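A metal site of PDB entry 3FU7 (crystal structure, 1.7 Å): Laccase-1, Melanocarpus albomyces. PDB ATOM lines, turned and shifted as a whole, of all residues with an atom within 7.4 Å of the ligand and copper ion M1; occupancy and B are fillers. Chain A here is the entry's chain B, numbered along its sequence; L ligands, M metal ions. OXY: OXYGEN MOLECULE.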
ATOM      1  N   HIS A  93     -21.845  -4.667   2.587  1.00  0.00           N
ATOM      2  CA  HIS A  93     -21.087  -3.985   3.597  1.00  0.00           C
ATOM      3  C   HIS A  93     -20.844  -4.914   4.782  1.00  0.00           C
ATOM      4  O   HIS A  93     -21.745  -5.651   5.194  1.00  0.00           O
ATOM      5  CB  HIS A  93     -21.843  -2.731   4.066  1.00  0.00           C
ATOM      6  CG  HIS A  93     -21.251  -2.089   5.275  1.00  0.00           C
ATOM      7  ND1 HIS A  93     -19.932  -1.695   5.320  1.00  0.00           N
ATOM      8  CD2 HIS A  93     -21.781  -1.806   6.485  1.00  0.00           C
ATOM      9  CE1 HIS A  93     -19.687  -1.168   6.507  1.00  0.00           C
ATOM     10  NE2 HIS A  93     -20.781  -1.226   7.228  1.00  0.00           N
ATOM     11  N   TRP A  94     -19.634  -4.870   5.338  1.00  0.00           N
ATOM     12  CA  TRP A  94     -19.192  -5.802   6.393  1.00  0.00           C
ATOM     13  C   TRP A  94     -19.208  -4.994   7.673  1.00  0.00           C
ATOM     14  O   TRP A  94     -18.255  -4.303   8.022  1.00  0.00           O
ATOM     15  CB  TRP A  94     -17.786  -6.351   6.027  1.00  0.00           C
ATOM     16  CG  TRP A  94     -17.744  -6.724   4.569  1.00  0.00           C
ATOM     17  CD1 TRP A  94     -17.330  -5.923   3.530  1.00  0.00           C
ATOM     18  CD2 TRP A  94     -18.248  -7.935   3.949  1.00  0.00           C
ATOM     19  NE1 TRP A  94     -17.492  -6.574   2.335  1.00  0.00           N
ATOM     20  CE2 TRP A  94     -18.074  -7.798   2.550  1.00  0.00           C
ATOM     21  CE3 TRP A  94     -18.806  -9.127   4.445  1.00  0.00           C
ATOM     22  CZ2 TRP A  94     -18.428  -8.805   1.639  1.00  0.00           C
ATOM     23  CZ3 TRP A  94     -19.177 -10.127   3.541  1.00  0.00           C
ATOM     24  CH2 TRP A  94     -18.988  -9.950   2.138  1.00  0.00           C
ATOM     25  N   HIS A  95     -20.350  -5.055   8.337  1.00  0.00           N
ATOM     26  CA  HIS A  95     -20.653  -4.133   9.425  1.00  0.00           C
ATOM     27  C   HIS A  95     -19.842  -4.490  10.654  1.00  0.00           C
ATOM     28  O   HIS A  95     -20.006  -5.582  11.215  1.00  0.00           O
ATOM     29  CB  HIS A  95     -22.150  -4.171   9.711  1.00  0.00           C
ATOM     30  CG  HIS A  95     -22.556  -3.290  10.844  1.00  0.00           C
ATOM     31  ND1 HIS A  95     -23.622  -2.432  10.767  1.00  0.00           N
ATOM     32  CD2 HIS A  95     -22.063  -3.160  12.103  1.00  0.00           C
ATOM     33  CE1 HIS A  95     -23.764  -1.793  11.913  1.00  0.00           C
ATOM     34  NE2 HIS A  95     -22.819  -2.216  12.745  1.00  0.00           N
ATOM     35  N   GLY A  96     -18.966  -3.582  11.075  1.00  0.00           N
ATOM     36  CA  GLY A  96     -18.128  -3.858  12.230  1.00  0.00           C
ATOM     37  C   GLY A  96     -16.711  -4.223  11.847  1.00  0.00           C
ATOM     38  O   GLY A  96     -15.846  -4.332  12.704  1.00  0.00           O
ATOM     39  N   ASP A 106     -15.194  -1.723   1.582  1.00  0.00           N
ATOM     40  CA  ASP A 106     -16.227  -1.420   2.595  1.00  0.00           C
ATOM     41  C   ASP A 106     -17.664  -1.665   2.140  1.00  0.00           C
ATOM     42  O   ASP A 106     -18.545  -1.886   2.951  1.00  0.00           O
ATOM     43  CB  ASP A 106     -16.055   0.019   3.106  1.00  0.00           C
ATOM     44  CG  ASP A 106     -16.878   0.317   4.348  1.00  0.00           C
ATOM     45  OD1 ASP A 106     -16.810  -0.459   5.322  1.00  0.00           O
ATOM     46  OD2 ASP A 106     -17.509   1.406   4.364  1.00  0.00           O
ATOM     47  N   GLY A 107     -17.894  -1.664   0.824  1.00  0.00           N
ATOM     48  CA  GLY A 107     -19.206  -2.031   0.290  1.00  0.00           C
ATOM     49  C   GLY A 107     -20.255  -0.925   0.425  1.00  0.00           C
ATOM     50  O   GLY A 107     -21.443  -1.202   0.381  1.00  0.00           O
ATOM     51  N   ALA A 108     -19.805   0.308   0.581  1.00  0.00           N
ATOM     52  CA  ALA A 108     -20.709   1.458   0.631  1.00  0.00           C
ATOM     53  C   ALA A 108     -20.880   2.027  -0.776  1.00  0.00           C
ATOM     54  O   ALA A 108     -20.106   2.857  -1.195  1.00  0.00           O
ATOM     55  CB  ALA A 108     -20.167   2.532   1.564  1.00  0.00           C
ATOM     56  N   TRP A 136     -21.783  -8.649  11.320  1.00  0.00           N
ATOM     57  CA  TRP A 136     -22.796  -9.013  10.328  1.00  0.00           C
ATOM     58  C   TRP A 136     -22.519  -8.290   9.035  1.00  0.00           C
ATOM     59  O   TRP A 136     -21.618  -7.446   8.963  1.00  0.00           O
ATOM     60  CB  TRP A 136     -24.223  -8.746  10.839  1.00  0.00           C
ATOM     61  CG  TRP A 136     -24.639  -7.328  11.100  1.00  0.00           C
ATOM     62  CD1 TRP A 136     -24.081  -6.426  11.964  1.00  0.00           C
ATOM     63  CD2 TRP A 136     -25.772  -6.697  10.528  1.00  0.00           C
ATOM     64  NE1 TRP A 136     -24.803  -5.238  11.938  1.00  0.00           N
ATOM     65  CE2 TRP A 136     -25.845  -5.374  11.068  1.00  0.00           C
ATOM     66  CE3 TRP A 136     -26.738  -7.109   9.614  1.00  0.00           C
ATOM     67  CZ2 TRP A 136     -26.843  -4.463  10.709  1.00  0.00           C
ATOM     68  CZ3 TRP A 136     -27.750  -6.200   9.252  1.00  0.00           C
ATOM     69  CH2 TRP A 136     -27.801  -4.892   9.806  1.00  0.00           C
ATOM     70  N   HIS A 138     -24.522  -6.888   5.187  1.00  0.00           N
ATOM     71  CA  HIS A 138     -25.807  -6.612   4.579  1.00  0.00           C
ATOM     72  C   HIS A 138     -25.568  -5.780   3.337  1.00  0.00           C
ATOM     73  O   HIS A 138     -24.569  -5.063   3.266  1.00  0.00           O
ATOM     74  CB  HIS A 138     -26.741  -5.849   5.562  1.00  0.00           C
ATOM     75  CG  HIS A 138     -26.151  -4.598   6.151  1.00  0.00           C
ATOM     76  ND1 HIS A 138     -26.163  -3.398   5.475  1.00  0.00           N
ATOM     77  CD2 HIS A 138     -25.598  -4.352   7.355  1.00  0.00           C
ATOM     78  CE1 HIS A 138     -25.609  -2.458   6.236  1.00  0.00           C
ATOM     79  NE2 HIS A 138     -25.245  -3.026   7.379  1.00  0.00           N
ATOM     80  N   SER A 139     -26.482  -5.845   2.368  1.00  0.00           N
ATOM     81  CA  SER A 139     -26.480  -4.898   1.224  1.00  0.00           C
ATOM     82  C   SER A 139     -26.524  -3.462   1.721  1.00  0.00           C
ATOM     83  O   SER A 139     -27.110  -3.158   2.772  1.00  0.00           O
ATOM     84  CB  SER A 139     -27.702  -5.136   0.329  1.00  0.00           C
ATOM     85  OG  SER A 139     -27.748  -4.185  -0.712  1.00  0.00           O
ATOM     86  N   HIS A 140     -25.892  -2.562   0.998  1.00  0.00           N
ATOM     87  CA  HIS A 140     -26.062  -1.141   1.315  1.00  0.00           C
ATOM     88  C   HIS A 140     -26.738  -0.411   0.151  1.00  0.00           C
ATOM     89  O   HIS A 140     -26.677   0.811   0.079  1.00  0.00           O
ATOM     90  CB  HIS A 140     -24.711  -0.485   1.597  1.00  0.00           C
ATOM     91  CG  HIS A 140     -24.697   0.367   2.823  1.00  0.00           C
ATOM     92  ND1 HIS A 140     -25.670   1.298   3.094  1.00  0.00           N
ATOM     93  CD2 HIS A 140     -23.847   0.389   3.876  1.00  0.00           C
ATOM     94  CE1 HIS A 140     -25.401   1.889   4.244  1.00  0.00           C
ATOM     95  NE2 HIS A 140     -24.295   1.359   4.734  1.00  0.00           N
ATOM     96  N   TYR A 145     -31.337  -4.671   2.002  1.00  0.00           N
ATOM     97  CA  TYR A 145     -31.091  -5.723   3.013  1.00  0.00           C
ATOM     98  C   TYR A 145     -32.370  -6.193   3.700  1.00  0.00           C
ATOM     99  O   TYR A 145     -32.449  -7.344   4.134  1.00  0.00           O
ATOM    100  CB  TYR A 145     -29.954  -5.385   3.993  1.00  0.00           C
ATOM    101  CG  TYR A 145     -30.231  -4.550   5.233  1.00  0.00           C
ATOM    102  CD1 TYR A 145     -30.588  -5.159   6.442  1.00  0.00           C
ATOM    103  CD2 TYR A 145     -30.008  -3.177   5.234  1.00  0.00           C
ATOM    104  CE1 TYR A 145     -30.791  -4.404   7.603  1.00  0.00           C
ATOM    105  CE2 TYR A 145     -30.192  -2.407   6.396  1.00  0.00           C
ATOM    106  CZ  TYR A 145     -30.556  -3.031   7.577  1.00  0.00           C
ATOM    107  OH  TYR A 145     -30.738  -2.294   8.721  1.00  0.00           O
ATOM    108  N   HIS A 434     -24.321   4.806  13.548  1.00  0.00           N
ATOM    109  CA  HIS A 434     -23.299   3.821  13.225  1.00  0.00           C
ATOM    110  C   HIS A 434     -22.180   4.434  12.372  1.00  0.00           C
ATOM    111  O   HIS A 434     -22.470   5.143  11.406  1.00  0.00           O
ATOM    112  CB  HIS A 434     -23.943   2.665  12.465  1.00  0.00           C
ATOM    113  CG  HIS A 434     -22.947   1.746  11.844  1.00  0.00           C
ATOM    114  ND1 HIS A 434     -21.976   1.108  12.593  1.00  0.00           N
ATOM    115  CD2 HIS A 434     -22.752   1.370  10.562  1.00  0.00           C
ATOM    116  CE1 HIS A 434     -21.224   0.370  11.789  1.00  0.00           C
ATOM    117  NE2 HIS A 434     -21.677   0.509  10.552  1.00  0.00           N
ATOM    118  N   LEU A 435     -20.938   4.169  12.754  1.00  0.00           N
ATOM    119  CA  LEU A 435     -19.739   4.669  12.069  1.00  0.00           C
ATOM    120  C   LEU A 435     -19.021   3.549  11.341  1.00  0.00           C
ATOM    121  O   LEU A 435     -18.715   2.526  11.934  1.00  0.00           O
ATOM    122  CB  LEU A 435     -18.772   5.287  13.085  1.00  0.00           C
ATOM    123  CG  LEU A 435     -17.492   5.922  12.542  1.00  0.00           C
ATOM    124  CD1 LEU A 435     -17.748   7.041  11.554  1.00  0.00           C
ATOM    125  CD2 LEU A 435     -16.663   6.429  13.758  1.00  0.00           C
ATOM    126  N   HIS A 436     -18.765   3.758  10.066  1.00  0.00           N
ATOM    127  CA  HIS A 436     -17.931   2.838   9.280  1.00  0.00           C
ATOM    128  C   HIS A 436     -16.443   3.130   9.558  1.00  0.00           C
ATOM    129  O   HIS A 436     -16.098   4.257   9.932  1.00  0.00           O
ATOM    130  CB  HIS A 436     -18.143   3.066   7.779  1.00  0.00           C
ATOM    131  CG  HIS A 436     -19.464   2.595   7.244  1.00  0.00           C
ATOM    132  ND1 HIS A 436     -19.576   1.998   6.002  1.00  0.00           N
ATOM    133  CD2 HIS A 436     -20.721   2.683   7.733  1.00  0.00           C
ATOM    134  CE1 HIS A 436     -20.850   1.728   5.771  1.00  0.00           C
ATOM    135  NE2 HIS A 436     -21.560   2.115   6.806  1.00  0.00           N
ATOM    136  N   THR A 478     -21.909   1.205  17.034  1.00  0.00           N
ATOM    137  CA  THR A 478     -23.263   1.710  16.982  1.00  0.00           C
ATOM    138  C   THR A 478     -23.710   2.095  18.401  1.00  0.00           C
ATOM    139  O   THR A 478     -23.474   1.320  19.332  1.00  0.00           O
ATOM    140  CB  THR A 478     -24.179   0.617  16.453  1.00  0.00           C
ATOM    141  OG1 THR A 478     -23.758   0.206  15.134  1.00  0.00           O
ATOM    142  CG2 THR A 478     -25.626   1.141  16.378  1.00  0.00           C
ATOM    143  N   LEU A 500     -18.909   6.317   5.881  1.00  0.00           N
ATOM    144  CA  LEU A 500     -20.235   6.822   6.259  1.00  0.00           C
ATOM    145  C   LEU A 500     -20.429   6.832   7.772  1.00  0.00           C
ATOM    146  O   LEU A 500     -19.880   5.980   8.500  1.00  0.00           O
ATOM    147  CB  LEU A 500     -21.343   5.968   5.643  1.00  0.00           C
ATOM    148  CG  LEU A 500     -21.446   5.940   4.131  1.00  0.00           C
ATOM    149  CD1 LEU A 500     -22.510   4.928   3.695  1.00  0.00           C
ATOM    150  CD2 LEU A 500     -21.833   7.319   3.687  1.00  0.00           C
ATOM    151  N   PHE A 501     -21.248   7.783   8.226  1.00  0.00           N
ATOM    152  CA  PHE A 501     -21.693   7.831   9.627  1.00  0.00           C
ATOM    153  C   PHE A 501     -23.189   8.167   9.538  1.00  0.00           C
ATOM    154  O   PHE A 501     -23.550   9.245   9.067  1.00  0.00           O
ATOM    155  CB  PHE A 501     -20.914   8.905  10.375  1.00  0.00           C
ATOM    156  CG  PHE A 501     -21.413   9.157  11.777  1.00  0.00           C
ATOM    157  CD1 PHE A 501     -21.392   8.153  12.726  1.00  0.00           C
ATOM    158  CD2 PHE A 501     -21.912  10.408  12.115  1.00  0.00           C
ATOM    159  CE1 PHE A 501     -21.878   8.397  14.024  1.00  0.00           C
ATOM    160  CE2 PHE A 501     -22.407  10.649  13.424  1.00  0.00           C
ATOM    161  CZ  PHE A 501     -22.387   9.630  14.357  1.00  0.00           C
ATOM    162  N   HIS A 502     -24.035   7.237   9.971  1.00  0.00           N
ATOM    163  CA  HIS A 502     -25.444   7.332   9.607  1.00  0.00           C
ATOM    164  C   HIS A 502     -26.352   6.654  10.617  1.00  0.00           C
ATOM    165  O   HIS A 502     -25.924   5.773  11.360  1.00  0.00           O
ATOM    166  CB  HIS A 502     -25.685   6.752   8.203  1.00  0.00           C
ATOM    167  CG  HIS A 502     -25.454   5.278   8.057  1.00  0.00           C
ATOM    168  ND1 HIS A 502     -26.430   4.336   8.327  1.00  0.00           N
ATOM    169  CD2 HIS A 502     -24.366   4.595   7.648  1.00  0.00           C
ATOM    170  CE1 HIS A 502     -25.933   3.125   8.083  1.00  0.00           C
ATOM    171  NE2 HIS A 502     -24.689   3.249   7.687  1.00  0.00           N
ATOM    172  N   CYS A 503     -27.618   7.088  10.649  1.00  0.00           N
ATOM    173  CA  CYS A 503     -28.618   6.353  11.410  1.00  0.00           C
ATOM    174  C   CYS A 503     -28.815   4.995  10.700  1.00  0.00           C
ATOM    175  O   CYS A 503     -28.869   4.930   9.456  1.00  0.00           O
ATOM    176  CB  CYS A 503     -29.947   7.122  11.431  1.00  0.00           C
ATOM    177  SG  CYS A 503     -31.265   6.122  12.136  1.00  0.00           S
ATOM    178  N   HIS A 504     -28.905   3.910  11.461  1.00  0.00           N
ATOM    179  CA  HIS A 504     -29.071   2.599  10.809  1.00  0.00           C
ATOM    180  C   HIS A 504     -30.547   2.215  10.651  1.00  0.00           C
ATOM    181  O   HIS A 504     -30.859   1.086  10.219  1.00  0.00           O
ATOM    182  CB  HIS A 504     -28.321   1.526  11.599  1.00  0.00           C
ATOM    183  CG  HIS A 504     -27.711   0.472  10.742  1.00  0.00           C
ATOM    184  ND1 HIS A 504     -28.476  -0.451  10.041  1.00  0.00           N
ATOM    185  CD2 HIS A 504     -26.424   0.182  10.474  1.00  0.00           C
ATOM    186  CE1 HIS A 504     -27.662  -1.253   9.369  1.00  0.00           C
ATOM    187  NE2 HIS A 504     -26.419  -0.886   9.624  1.00  0.00           N
ATOM    188  N   VAL A 509     -31.906   6.585   6.893  1.00  0.00           N
ATOM    189  CA  VAL A 509     -30.724   6.778   6.023  1.00  0.00           C
ATOM    190  C   VAL A 509     -31.165   6.874   4.551  1.00  0.00           C
ATOM    191  O   VAL A 509     -30.577   7.635   3.777  1.00  0.00           O
ATOM    192  CB  VAL A 509     -29.601   5.751   6.297  1.00  0.00           C
ATOM    193  CG1 VAL A 509     -30.098   4.318   6.088  1.00  0.00           C
ATOM    194  CG2 VAL A 509     -28.350   6.057   5.452  1.00  0.00           C
ATOM    195  N   SER A 514     -27.329  10.861   6.990  1.00  0.00           N
ATOM    196  CA  SER A 514     -25.934  10.422   7.022  1.00  0.00           C
ATOM    197  C   SER A 514     -25.022  11.584   6.742  1.00  0.00           C
ATOM    198  O   SER A 514     -25.451  12.583   6.127  1.00  0.00           O
ATOM    199  CB  SER A 514     -25.713   9.384   5.907  1.00  0.00           C
ATOM    200  OG  SER A 514     -24.439   8.782   5.977  1.00  0.00           O
ATOM    201  N   LEU A 559     -28.584   4.823  -0.072  1.00  0.00           N
ATOM    202  CA  LEU A 559     -27.900   4.138   1.038  1.00  0.00           C
ATOM    203  C   LEU A 559     -28.831   3.410   1.987  1.00  0.00           C
ATOM    204  O   LEU A 559     -30.040   3.681   1.957  1.00  0.00           O
ATOM    205  CB  LEU A 559     -27.107   5.166   1.840  1.00  0.00           C
ATOM    206  CG  LEU A 559     -25.918   5.837   1.153  1.00  0.00           C
ATOM    207  CD1 LEU A 559     -25.389   6.973   2.048  1.00  0.00           C
ATOM    208  CD2 LEU A 559     -24.786   4.881   0.842  1.00  0.00           C
ATOM    209  OXT LEU A 559     -28.364   2.598   2.810  1.00  0.00           O
HETATM  210  O1  OXY L   1     -24.733   0.013   7.554  1.00  0.00           O
HETATM  211  O2  OXY L   1     -23.767   0.118   8.018  1.00  0.00           O
HETATM  212 CU    CU M   1     -23.535   1.962   6.612  1.00  0.00          CU
HETATM  213 CU    CU M   2     -24.793  -2.122   9.136  1.00  0.00          CU
HETATM  214 CU    CU M   3     -21.142  -0.414   8.933  1.00  0.00          CU
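OG1 of Thr 478 sits at hydrogen-bond distance from ND1 of His 434, at 3.2 Å.
The backbone carbonyl oxygen of His 138 sits at hydrogen-bond distance from the backbone NH of His 93, at 2.8 Å.
The backbone carbonyl oxygen (O) of Trp 136 sits at hydrogen-bond distance from the backbone NH (N) of His 95 (2.8 Å).
A ring nitrogen (ND1) of His 93 sits at hydrogen-bond distance from the backbone carbonyl oxygen (O) of Asp 106, at 2.8 Å.
ND1 of His 436 is in hydrogen-bond range of OD2 of Asp 106.
ND1 of His 504 is in hydrogen-bond range of OH of Tyr 145 (3.2 Å).
ND1 of His 434 sits close to NE2 of His 95.
A ring nitrogen (ND1) of His 140 is in hydrogen-bond range of the chain-end carboxylate (OXT) of Leu 559 (3.0 Å).
A ring nitrogen (NE2) of His 93 sits close to an oxygen (O2) of the ligand, at 3.4 Å.
An oxygen (O1) of the ligand sits close to a ring nitrogen (NE2) of His 138 (3.1 Å).
An oxygen (O2) of the ligand lies close to a ring nitrogen (NE2) of His 434, at 3.3 Å.
O1 of the ligand lies close to NE2 of His 504.
Residues that only touch the ligand: His 95.
Of the 24 residues printed, 8 come within 4 Å of the ligand.
Copper ion M1 is bound by NE2 of His 436 (2.0 Å), NE2 of His 502 (2.0 Å), NE2 of His 140 (2.1 Å) and O2 of the ligand (2.3 Å).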
